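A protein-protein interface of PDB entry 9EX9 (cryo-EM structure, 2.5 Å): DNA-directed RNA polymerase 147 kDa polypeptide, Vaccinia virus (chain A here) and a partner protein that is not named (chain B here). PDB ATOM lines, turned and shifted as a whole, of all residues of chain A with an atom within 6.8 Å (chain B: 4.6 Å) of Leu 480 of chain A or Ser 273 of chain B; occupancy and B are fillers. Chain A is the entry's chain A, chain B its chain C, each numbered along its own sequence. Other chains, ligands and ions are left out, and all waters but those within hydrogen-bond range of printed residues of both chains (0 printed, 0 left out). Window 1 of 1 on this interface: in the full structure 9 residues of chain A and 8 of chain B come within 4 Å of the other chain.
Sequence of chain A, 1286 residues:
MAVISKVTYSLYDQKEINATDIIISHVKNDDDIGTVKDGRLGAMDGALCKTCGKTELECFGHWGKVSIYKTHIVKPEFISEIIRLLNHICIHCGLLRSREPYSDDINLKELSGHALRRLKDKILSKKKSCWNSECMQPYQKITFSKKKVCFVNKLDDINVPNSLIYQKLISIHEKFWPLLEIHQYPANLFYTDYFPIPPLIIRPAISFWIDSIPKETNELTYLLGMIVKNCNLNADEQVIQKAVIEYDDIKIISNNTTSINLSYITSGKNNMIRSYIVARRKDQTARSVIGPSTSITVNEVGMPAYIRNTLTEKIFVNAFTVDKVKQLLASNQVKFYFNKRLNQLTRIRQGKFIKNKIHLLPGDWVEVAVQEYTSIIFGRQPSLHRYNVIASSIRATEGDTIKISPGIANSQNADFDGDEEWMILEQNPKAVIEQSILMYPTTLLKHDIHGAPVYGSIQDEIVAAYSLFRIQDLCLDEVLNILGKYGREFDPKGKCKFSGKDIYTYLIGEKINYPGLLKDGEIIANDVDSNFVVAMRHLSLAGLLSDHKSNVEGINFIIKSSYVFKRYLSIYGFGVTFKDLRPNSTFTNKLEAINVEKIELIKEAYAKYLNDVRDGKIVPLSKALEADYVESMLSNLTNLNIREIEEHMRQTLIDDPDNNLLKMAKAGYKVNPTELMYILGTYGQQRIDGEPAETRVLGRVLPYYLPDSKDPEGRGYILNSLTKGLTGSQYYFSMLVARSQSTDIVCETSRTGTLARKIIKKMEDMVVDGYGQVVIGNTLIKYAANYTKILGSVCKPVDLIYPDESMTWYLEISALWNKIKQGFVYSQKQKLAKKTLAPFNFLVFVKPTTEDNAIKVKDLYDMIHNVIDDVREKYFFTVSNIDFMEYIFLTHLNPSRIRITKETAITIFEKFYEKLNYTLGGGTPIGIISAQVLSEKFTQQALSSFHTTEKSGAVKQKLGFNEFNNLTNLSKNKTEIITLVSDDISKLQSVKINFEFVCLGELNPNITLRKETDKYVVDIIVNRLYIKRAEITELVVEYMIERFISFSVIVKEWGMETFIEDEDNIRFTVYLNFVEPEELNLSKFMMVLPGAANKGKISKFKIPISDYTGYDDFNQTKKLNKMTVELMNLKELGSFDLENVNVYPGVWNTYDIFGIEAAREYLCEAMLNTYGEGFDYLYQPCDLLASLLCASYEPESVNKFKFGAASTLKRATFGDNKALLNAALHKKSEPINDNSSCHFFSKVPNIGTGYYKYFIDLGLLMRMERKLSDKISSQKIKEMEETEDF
Among the printed residues, pairs that only touch across the chains: Leu 480 of chain A with Ser 273 of chain B (3.9 Å), Leu 480 of chain A with Tyr 274 of chain B (3.1 Å), Asn 481 of chain A with Ser 269 of chain B (3.7 Å), Gly 484 of chain A with Glu 272 of chain B (3.5 Å), Gly 484 of chain A with Tyr 274 of chain B (3.7 Å), Lys 485 of chain A with Glu 272 of chain B (3.7 Å) and Lys 485 of chain A with Tyr 274 of chain B (3.9 Å).
Cys 475 of chain A touches none of the printed residues of chain B. Leu 480 of chain A touches two residues of chain B. Leu 483 of chain A touches none of the printed residues of chain B. Of the printed residues of chain B, Gly 484 of chain A touches Glu 272 and Tyr 274. Of the printed residues of chain B, Lys 485 of chain A touches Glu 272 (3.7 Å) and Tyr 274 (3.9 Å). Printed residues of chain B within 4 Å of Arg 488 of chain A: Tyr 274 (3.2 Å). Of the printed residues of chain A, Arg 270 of chain B touches Asn 481 (3.0 Å). Of the printed residues of chain A, Tyr 274 of chain B touches Leu 480, Gly 484, Lys 485 and Arg 488. The nearest residue of chain B that does not touch Leu 480 of chain A is His 275 of chain B (4.05 Å). The nearest residue of chain A that does not touch Ser 273 of chain B is Gly 484 of chain A (4.4 Å).
The side-chain amide nitrogen (ND2) of Asn 481 of chain A lies close to the backbone carbonyl oxygen (O) of Asp 477 of chain A. The backbone carbonyl oxygen of Asn 481 of chain A sits at hydrogen-bond distance from the guanidinium group of Arg 567 of chain A (3.0 Å). O of Ile 482 of chain A lies close to NE of Arg 567 of chain A (3.4 Å). N of Glu 272 of chain B sits close to O of Val 253 of chain B (3.4 Å). The backbone carbonyl oxygen (O) of Ser 273 of chain B is in hydrogen-bond range of the backbone NH (N) of Val 253 of chain B (2.9 Å). The side-chain hydroxyl of Ser 273 of chain B is in hydrogen-bond range of the backbone carbonyl oxygen of Arg 270 of chain B (3.0 Å).
The side-chain carboxylate (OD1) of Asp 477 of chain A sits at hydrogen-bond distance from a ring nitrogen (ND1) of His 275 of chain B, at 2.5 Å. N of Arg 270 of chain B is in hydrogen-bond range of OD1 of Asn 481 of chain A (3.0 Å). OD1 of Asn 481 of chain A is in hydrogen-bond range of OG of Ser 273 of chain B (3.5 Å). The side-chain amide oxygen (OD1) of Asn 481 of chain A is in hydrogen-bond range of a ring nitrogen (NE2) of His 275 of chain B, at 3.2 Å. The side-chain hydroxyl of Tyr 274 of chain B sits at hydrogen-bond distance from the guanidinium group of Arg 488 of chain A, at 3.2 Å. The guanidinium group of Arg 567 of chain A is in salt-bridge range of the side-chain carboxylate of Glu 272 of chain B (3.6 Å).
Printed residues of chain A that touch a printed residue of chain B: Asp 477, Leu 480, Asn 481, Gly 484, Lys 485, Arg 488 and Arg 567. Hydrophobic or aromatic side chains of chain A that line the printed part of chain B: Leu 480. Printed residues of chain B that touch a printed residue of chain A: Ser 269, Arg 270, Glu 272, Ser 273, Tyr 274 and His 275. Hydrophobic or aromatic side chains of chain B within 4 Å of the printed part of chain A: Tyr 274 and His 275. Among the printed residues, Asp or Glu carboxylates within 4 Å of a Lys or Arg side-chain nitrogen of the other chain: Arg 567 of chain A with Glu 272 of chain B (3.6 Å).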
ATOM      1  N   CYS A 475      27.062  21.213  -7.727  1.00  0.00           N
ATOM      2  CA  CYS A 475      25.952  21.829  -7.026  1.00  0.00           C
ATOM      3  C   CYS A 475      24.924  22.312  -8.045  1.00  0.00           C
ATOM      4  O   CYS A 475      25.126  22.231  -9.257  1.00  0.00           O
ATOM      5  CB  CYS A 475      26.444  22.971  -6.144  1.00  0.00           C
ATOM      6  SG  CYS A 475      27.031  24.413  -7.035  1.00  0.00           S
ATOM      7  N   LEU A 476      23.793  22.814  -7.554  1.00  0.00           N
ATOM      8  CA  LEU A 476      22.739  23.249  -8.462  1.00  0.00           C
ATOM      9  C   LEU A 476      23.190  24.437  -9.306  1.00  0.00           C
ATOM     10  O   LEU A 476      22.872  24.517 -10.498  1.00  0.00           O
ATOM     11  CB  LEU A 476      21.481  23.595  -7.669  1.00  0.00           C
ATOM     12  CG  LEU A 476      20.256  23.959  -8.506  1.00  0.00           C
ATOM     13  CD1 LEU A 476      19.852  22.809  -9.402  1.00  0.00           C
ATOM     14  CD2 LEU A 476      19.110  24.360  -7.612  1.00  0.00           C
ATOM     15  N   ASP A 477      23.933  25.368  -8.707  1.00  0.00           N
ATOM     16  CA  ASP A 477      24.368  26.548  -9.445  1.00  0.00           C
ATOM     17  C   ASP A 477      25.259  26.170 -10.619  1.00  0.00           C
ATOM     18  O   ASP A 477      25.141  26.744 -11.703  1.00  0.00           O
ATOM     19  CB  ASP A 477      25.096  27.515  -8.514  1.00  0.00           C
ATOM     20  CG  ASP A 477      24.155  28.485  -7.828  1.00  0.00           C
ATOM     21  OD1 ASP A 477      23.167  28.907  -8.458  1.00  0.00           O
ATOM     22  OD2 ASP A 477      24.407  28.833  -6.658  1.00  0.00           O
ATOM     23  N   GLU A 478      26.161  25.209 -10.426  1.00  0.00           N
ATOM     24  CA  GLU A 478      27.034  24.794 -11.518  1.00  0.00           C
ATOM     25  C   GLU A 478      26.253  24.076 -12.611  1.00  0.00           C
ATOM     26  O   GLU A 478      26.527  24.262 -13.803  1.00  0.00           O
ATOM     27  CB  GLU A 478      28.149  23.912 -10.971  1.00  0.00           C
ATOM     28  CG  GLU A 478      29.055  24.650 -10.013  1.00  0.00           C
ATOM     29  CD  GLU A 478      29.995  23.734  -9.274  1.00  0.00           C
ATOM     30  OE1 GLU A 478      29.759  22.513  -9.279  1.00  0.00           O
ATOM     31  OE2 GLU A 478      30.974  24.234  -8.687  1.00  0.00           O
ATOM     32  N   VAL A 479      25.273  23.259 -12.230  1.00  0.00           N
ATOM     33  CA  VAL A 479      24.426  22.620 -13.231  1.00  0.00           C
ATOM     34  C   VAL A 479      23.721  23.672 -14.069  1.00  0.00           C
ATOM     35  O   VAL A 479      23.663  23.572 -15.299  1.00  0.00           O
ATOM     36  CB  VAL A 479      23.421  21.675 -12.555  1.00  0.00           C
ATOM     37  CG1 VAL A 479      22.420  21.164 -13.568  1.00  0.00           C
ATOM     38  CG2 VAL A 479      24.141  20.524 -11.903  1.00  0.00           C
ATOM     39  N   LEU A 480      23.177  24.703 -13.420  1.00  0.00           N
ATOM     40  CA  LEU A 480      22.474  25.742 -14.162  1.00  0.00           C
ATOM     41  C   LEU A 480      23.425  26.583 -15.005  1.00  0.00           C
ATOM     42  O   LEU A 480      23.050  27.026 -16.095  1.00  0.00           O
ATOM     43  CB  LEU A 480      21.683  26.620 -13.197  1.00  0.00           C
ATOM     44  CG  LEU A 480      20.562  25.899 -12.444  1.00  0.00           C
ATOM     45  CD1 LEU A 480      19.921  26.815 -11.429  1.00  0.00           C
ATOM     46  CD2 LEU A 480      19.518  25.374 -13.402  1.00  0.00           C
ATOM     47  N   ASN A 481      24.649  26.813 -14.528  1.00  0.00           N
ATOM     48  CA  ASN A 481      25.646  27.502 -15.340  1.00  0.00           C
ATOM     49  C   ASN A 481      25.943  26.729 -16.613  1.00  0.00           C
ATOM     50  O   ASN A 481      26.074  27.317 -17.690  1.00  0.00           O
ATOM     51  CB  ASN A 481      26.932  27.704 -14.544  1.00  0.00           C
ATOM     52  CG  ASN A 481      26.857  28.874 -13.602  1.00  0.00           C
ATOM     53  OD1 ASN A 481      26.100  29.813 -13.826  1.00  0.00           O
ATOM     54  ND2 ASN A 481      27.652  28.834 -12.543  1.00  0.00           N
ATOM     55  N   ILE A 482      26.073  25.407 -16.508  1.00  0.00           N
ATOM     56  CA  ILE A 482      26.258  24.597 -17.709  1.00  0.00           C
ATOM     57  C   ILE A 482      25.037  24.706 -18.614  1.00  0.00           C
ATOM     58  O   ILE A 482      25.158  24.931 -19.821  1.00  0.00           O
ATOM     59  CB  ILE A 482      26.545  23.131 -17.337  1.00  0.00           C
ATOM     60  CG1 ILE A 482      27.939  23.000 -16.729  1.00  0.00           C
ATOM     61  CG2 ILE A 482      26.413  22.243 -18.561  1.00  0.00           C
ATOM     62  CD1 ILE A 482      28.262  21.615 -16.238  1.00  0.00           C
ATOM     63  N   LEU A 483      23.842  24.559 -18.039  1.00  0.00           N
ATOM     64  CA  LEU A 483      22.633  24.457 -18.853  1.00  0.00           C
ATOM     65  C   LEU A 483      22.344  25.746 -19.608  1.00  0.00           C
ATOM     66  O   LEU A 483      21.978  25.708 -20.786  1.00  0.00           O
ATOM     67  CB  LEU A 483      21.442  24.078 -17.978  1.00  0.00           C
ATOM     68  CG  LEU A 483      21.375  22.614 -17.556  1.00  0.00           C
ATOM     69  CD1 LEU A 483      20.286  22.410 -16.532  1.00  0.00           C
ATOM     70  CD2 LEU A 483      21.141  21.731 -18.761  1.00  0.00           C
ATOM     71  N   GLY A 484      22.491  26.893 -18.957  1.00  0.00           N
ATOM     72  CA  GLY A 484      22.259  28.141 -19.659  1.00  0.00           C
ATOM     73  C   GLY A 484      20.780  28.425 -19.815  1.00  0.00           C
ATOM     74  O   GLY A 484      19.993  28.284 -18.875  1.00  0.00           O
ATOM     75  N   LYS A 485      20.391  28.838 -21.022  1.00  0.00           N
ATOM     76  CA  LYS A 485      19.014  29.246 -21.270  1.00  0.00           C
ATOM     77  C   LYS A 485      18.042  28.079 -21.305  1.00  0.00           C
ATOM     78  O   LYS A 485      16.832  28.312 -21.337  1.00  0.00           O
ATOM     79  CB  LYS A 485      18.919  30.018 -22.583  1.00  0.00           C
ATOM     80  CG  LYS A 485      19.075  29.166 -23.823  1.00  0.00           C
ATOM     81  CD  LYS A 485      19.032  30.017 -25.070  1.00  0.00           C
ATOM     82  CE  LYS A 485      19.223  29.185 -26.316  1.00  0.00           C
ATOM     83  NZ  LYS A 485      19.444  30.031 -27.518  1.00  0.00           N
ATOM     84  N   TYR A 486      18.530  26.845 -21.314  1.00  0.00           N
ATOM     85  CA  TYR A 486      17.673  25.670 -21.251  1.00  0.00           C
ATOM     86  C   TYR A 486      17.465  25.170 -19.832  1.00  0.00           C
ATOM     87  O   TYR A 486      16.884  24.099 -19.650  1.00  0.00           O
ATOM     88  CB  TYR A 486      18.256  24.537 -22.096  1.00  0.00           C
ATOM     89  CG  TYR A 486      18.274  24.824 -23.571  1.00  0.00           C
ATOM     90  CD1 TYR A 486      17.129  24.691 -24.333  1.00  0.00           C
ATOM     91  CD2 TYR A 486      19.435  25.222 -24.202  1.00  0.00           C
ATOM     92  CE1 TYR A 486      17.142  24.951 -25.677  1.00  0.00           C
ATOM     93  CE2 TYR A 486      19.454  25.484 -25.546  1.00  0.00           C
ATOM     94  CZ  TYR A 486      18.306  25.346 -26.279  1.00  0.00           C
ATOM     95  OH  TYR A 486      18.324  25.609 -27.622  1.00  0.00           O
ATOM     96  N   GLY A 487      17.935  25.899 -18.833  1.00  0.00           N
ATOM     97  CA  GLY A 487      17.820  25.471 -17.462  1.00  0.00           C
ATOM     98  C   GLY A 487      16.581  25.930 -16.742  1.00  0.00           C
ATOM     99  O   GLY A 487      16.477  25.721 -15.532  1.00  0.00           O
ATOM    100  N   ARG A 488      15.630  26.561 -17.432  1.00  0.00           N
ATOM    101  CA  ARG A 488      14.438  27.038 -16.740  1.00  0.00           C
ATOM    102  C   ARG A 488      13.625  25.879 -16.184  1.00  0.00           C
ATOM    103  O   ARG A 488      13.170  25.928 -15.036  1.00  0.00           O
ATOM    104  CB  ARG A 488      13.574  27.881 -17.673  1.00  0.00           C
ATOM    105  CG  ARG A 488      12.475  28.634 -16.935  1.00  0.00           C
ATOM    106  CD  ARG A 488      11.311  29.000 -17.836  1.00  0.00           C
ATOM    107  NE  ARG A 488      11.654  30.036 -18.802  1.00  0.00           N
ATOM    108  CZ  ARG A 488      12.080  29.806 -20.037  1.00  0.00           C
ATOM    109  NH1 ARG A 488      12.250  28.576 -20.495  1.00  0.00           N
ATOM    110  NH2 ARG A 488      12.338  30.838 -20.835  1.00  0.00           N
ATOM    111  N   PHE A 490      14.596  22.779 -15.565  1.00  0.00           N
ATOM    112  CA  PHE A 490      15.302  21.764 -14.799  1.00  0.00           C
ATOM    113  C   PHE A 490      14.630  21.582 -13.448  1.00  0.00           C
ATOM    114  O   PHE A 490      14.196  22.547 -12.815  1.00  0.00           O
ATOM    115  CB  PHE A 490      16.765  22.152 -14.615  1.00  0.00           C
ATOM    116  CG  PHE A 490      17.575  21.118 -13.897  1.00  0.00           C
ATOM    117  CD1 PHE A 490      17.872  19.914 -14.503  1.00  0.00           C
ATOM    118  CD2 PHE A 490      18.041  21.348 -12.620  1.00  0.00           C
ATOM    119  CE1 PHE A 490      18.615  18.963 -13.849  1.00  0.00           C
ATOM    120  CE2 PHE A 490      18.785  20.399 -11.963  1.00  0.00           C
ATOM    121  CZ  PHE A 490      19.072  19.205 -12.579  1.00  0.00           C
ATOM    122  N   ARG A 567      28.745  25.386 -24.163  1.00  0.00           N
ATOM    123  CA  ARG A 567      28.847  26.036 -22.857  1.00  0.00           C
ATOM    124  C   ARG A 567      29.835  25.306 -21.949  1.00  0.00           C
ATOM    125  O   ARG A 567      30.562  25.940 -21.174  1.00  0.00           O
ATOM    126  CB  ARG A 567      27.475  26.140 -22.199  1.00  0.00           C
ATOM    127  CG  ARG A 567      26.712  27.375 -22.627  1.00  0.00           C
ATOM    128  CD  ARG A 567      25.466  27.594 -21.807  1.00  0.00           C
ATOM    129  NE  ARG A 567      25.729  28.209 -20.512  1.00  0.00           N
ATOM    130  CZ  ARG A 567      25.797  29.515 -20.299  1.00  0.00           C
ATOM    131  NH1 ARG A 567      25.694  30.383 -21.286  1.00  0.00           N
ATOM    132  NH2 ARG A 567      25.974  29.960 -19.061  1.00  0.00           N
ATOM    133  N   LEU B 251      15.886  33.932 -10.606  1.00  0.00           N
ATOM    134  CA  LEU B 251      16.538  35.089 -11.201  1.00  0.00           C
ATOM    135  C   LEU B 251      17.246  34.653 -12.474  1.00  0.00           C
ATOM    136  O   LEU B 251      18.037  33.707 -12.454  1.00  0.00           O
ATOM    137  CB  LEU B 251      17.534  35.704 -10.221  1.00  0.00           C
ATOM    138  CG  LEU B 251      18.391  36.867 -10.715  1.00  0.00           C
ATOM    139  CD1 LEU B 251      17.578  38.135 -10.819  1.00  0.00           C
ATOM    140  CD2 LEU B 251      19.564  37.067  -9.784  1.00  0.00           C
ATOM    141  N   PHE B 252      16.956  35.337 -13.572  1.00  0.00           N
ATOM    142  CA  PHE B 252      17.670  35.158 -14.827  1.00  0.00           C
ATOM    143  C   PHE B 252      18.732  36.246 -14.911  1.00  0.00           C
ATOM    144  O   PHE B 252      18.404  37.437 -14.976  1.00  0.00           O
ATOM    145  CB  PHE B 252      16.709  35.224 -16.010  1.00  0.00           C
ATOM    146  CG  PHE B 252      17.378  35.085 -17.341  1.00  0.00           C
ATOM    147  CD1 PHE B 252      17.990  33.902 -17.704  1.00  0.00           C
ATOM    148  CD2 PHE B 252      17.384  36.131 -18.237  1.00  0.00           C
ATOM    149  CE1 PHE B 252      18.600  33.771 -18.928  1.00  0.00           C
ATOM    150  CE2 PHE B 252      17.990  36.003 -19.460  1.00  0.00           C
ATOM    151  CZ  PHE B 252      18.599  34.822 -19.805  1.00  0.00           C
ATOM    152  N   VAL B 253      19.998  35.833 -14.887  1.00  0.00           N
ATOM    153  CA  VAL B 253      21.135  36.740 -14.972  1.00  0.00           C
ATOM    154  C   VAL B 253      21.588  36.797 -16.422  1.00  0.00           C
ATOM    155  O   VAL B 253      21.894  35.759 -17.026  1.00  0.00           O
ATOM    156  CB  VAL B 253      22.282  36.282 -14.064  1.00  0.00           C
ATOM    157  CG1 VAL B 253      23.450  37.226 -14.185  1.00  0.00           C
ATOM    158  CG2 VAL B 253      21.822  36.189 -12.632  1.00  0.00           C
ATOM    159  N   SER B 269      26.727  32.784 -10.247  1.00  0.00           N
ATOM    160  CA  SER B 269      26.070  32.835 -11.544  1.00  0.00           C
ATOM    161  C   SER B 269      27.033  33.170 -12.681  1.00  0.00           C
ATOM    162  O   SER B 269      28.091  33.766 -12.483  1.00  0.00           O
ATOM    163  CB  SER B 269      24.951  33.868 -11.514  1.00  0.00           C
ATOM    164  OG  SER B 269      25.439  35.108 -11.038  1.00  0.00           O
ATOM    165  N   ARG B 270      26.638  32.768 -13.889  1.00  0.00           N
ATOM    166  CA  ARG B 270      27.247  33.173 -15.147  1.00  0.00           C
ATOM    167  C   ARG B 270      26.281  34.097 -15.883  1.00  0.00           C
ATOM    168  O   ARG B 270      25.222  34.456 -15.367  1.00  0.00           O
ATOM    169  CB  ARG B 270      27.611  31.952 -15.992  1.00  0.00           C
ATOM    170  CG  ARG B 270      28.993  31.419 -15.741  1.00  0.00           C
ATOM    171  CD  ARG B 270      29.365  30.382 -16.774  1.00  0.00           C
ATOM    172  NE  ARG B 270      30.149  30.963 -17.855  1.00  0.00           N
ATOM    173  CZ  ARG B 270      31.462  31.142 -17.813  1.00  0.00           C
ATOM    174  NH1 ARG B 270      32.174  30.801 -16.754  1.00  0.00           N
ATOM    175  NH2 ARG B 270      32.077  31.677 -18.863  1.00  0.00           N
ATOM    176  N   LEU B 271      26.635  34.463 -17.110  1.00  0.00           N
ATOM    177  CA  LEU B 271      26.027  35.610 -17.767  1.00  0.00           C
ATOM    178  C   LEU B 271      24.810  35.276 -18.619  1.00  0.00           C
ATOM    179  O   LEU B 271      24.300  36.171 -19.297  1.00  0.00           O
ATOM    180  CB  LEU B 271      27.071  36.317 -18.635  1.00  0.00           C
ATOM    181  CG  LEU B 271      26.761  37.745 -19.081  1.00  0.00           C
ATOM    182  CD1 LEU B 271      26.550  38.646 -17.888  1.00  0.00           C
ATOM    183  CD2 LEU B 271      27.875  38.279 -19.952  1.00  0.00           C
ATOM    184  N   GLU B 272      24.338  34.036 -18.655  1.00  0.00           N
ATOM    185  CA  GLU B 272      23.079  33.743 -19.342  1.00  0.00           C
ATOM    186  C   GLU B 272      22.296  32.649 -18.621  1.00  0.00           C
ATOM    187  O   GLU B 272      21.813  31.703 -19.241  1.00  0.00           O
ATOM    188  CB  GLU B 272      23.342  33.351 -20.791  1.00  0.00           C
ATOM    189  CG  GLU B 272      22.126  33.406 -21.690  1.00  0.00           C
ATOM    190  CD  GLU B 272      22.381  32.761 -23.035  1.00  0.00           C
ATOM    191  OE1 GLU B 272      22.746  31.571 -23.065  1.00  0.00           O
ATOM    192  OE2 GLU B 272      22.229  33.444 -24.064  1.00  0.00           O
ATOM    193  N   SER B 273      22.163  32.743 -17.299  1.00  0.00           N
ATOM    194  CA  SER B 273      21.759  31.574 -16.524  1.00  0.00           C
ATOM    195  C   SER B 273      20.682  31.890 -15.495  1.00  0.00           C
ATOM    196  O   SER B 273      20.564  33.017 -15.016  1.00  0.00           O
ATOM    197  CB  SER B 273      22.961  30.965 -15.819  1.00  0.00           C
ATOM    198  OG  SER B 273      23.623  31.934 -15.036  1.00  0.00           O
ATOM    199  N   TYR B 274      19.905  30.863 -15.150  1.00  0.00           N
ATOM    200  CA  TYR B 274      18.897  30.939 -14.101  1.00  0.00           C
ATOM    201  C   TYR B 274      19.476  30.469 -12.775  1.00  0.00           C
ATOM    202  O   TYR B 274      20.319  29.571 -12.730  1.00  0.00           O
ATOM    203  CB  TYR B 274      17.681  30.074 -14.441  1.00  0.00           C
ATOM    204  CG  TYR B 274      16.935  30.499 -15.674  1.00  0.00           C
ATOM    205  CD1 TYR B 274      17.353  30.097 -16.927  1.00  0.00           C
ATOM    206  CD2 TYR B 274      15.808  31.292 -15.587  1.00  0.00           C
ATOM    207  CE1 TYR B 274      16.676  30.480 -18.056  1.00  0.00           C
ATOM    208  CE2 TYR B 274      15.125  31.682 -16.712  1.00  0.00           C
ATOM    209  CZ  TYR B 274      15.562  31.271 -17.943  1.00  0.00           C
ATOM    210  OH  TYR B 274      14.889  31.649 -19.076  1.00  0.00           O
ATOM    211  N   HIS B 275      19.013  31.079 -11.688  1.00  0.00           N
ATOM    212  CA  HIS B 275      19.475  30.695 -10.362  1.00  0.00           C
ATOM    213  C   HIS B 275      18.387  30.966  -9.337  1.00  0.00           C
ATOM    214  O   HIS B 275      17.588  31.894  -9.476  1.00  0.00           O
ATOM    215  CB  HIS B 275      20.760  31.436  -9.984  1.00  0.00           C
ATOM    216  CG  HIS B 275      21.922  31.090 -10.855  1.00  0.00           C
ATOM    217  ND1 HIS B 275      22.701  29.975 -10.643  1.00  0.00           N
ATOM    218  CD2 HIS B 275      22.422  31.694 -11.957  1.00  0.00           C
ATOM    219  CE1 HIS B 275      23.637  29.913 -11.572  1.00  0.00           C
ATOM    220  NE2 HIS B 275      23.489  30.945 -12.381  1.00  0.00           N
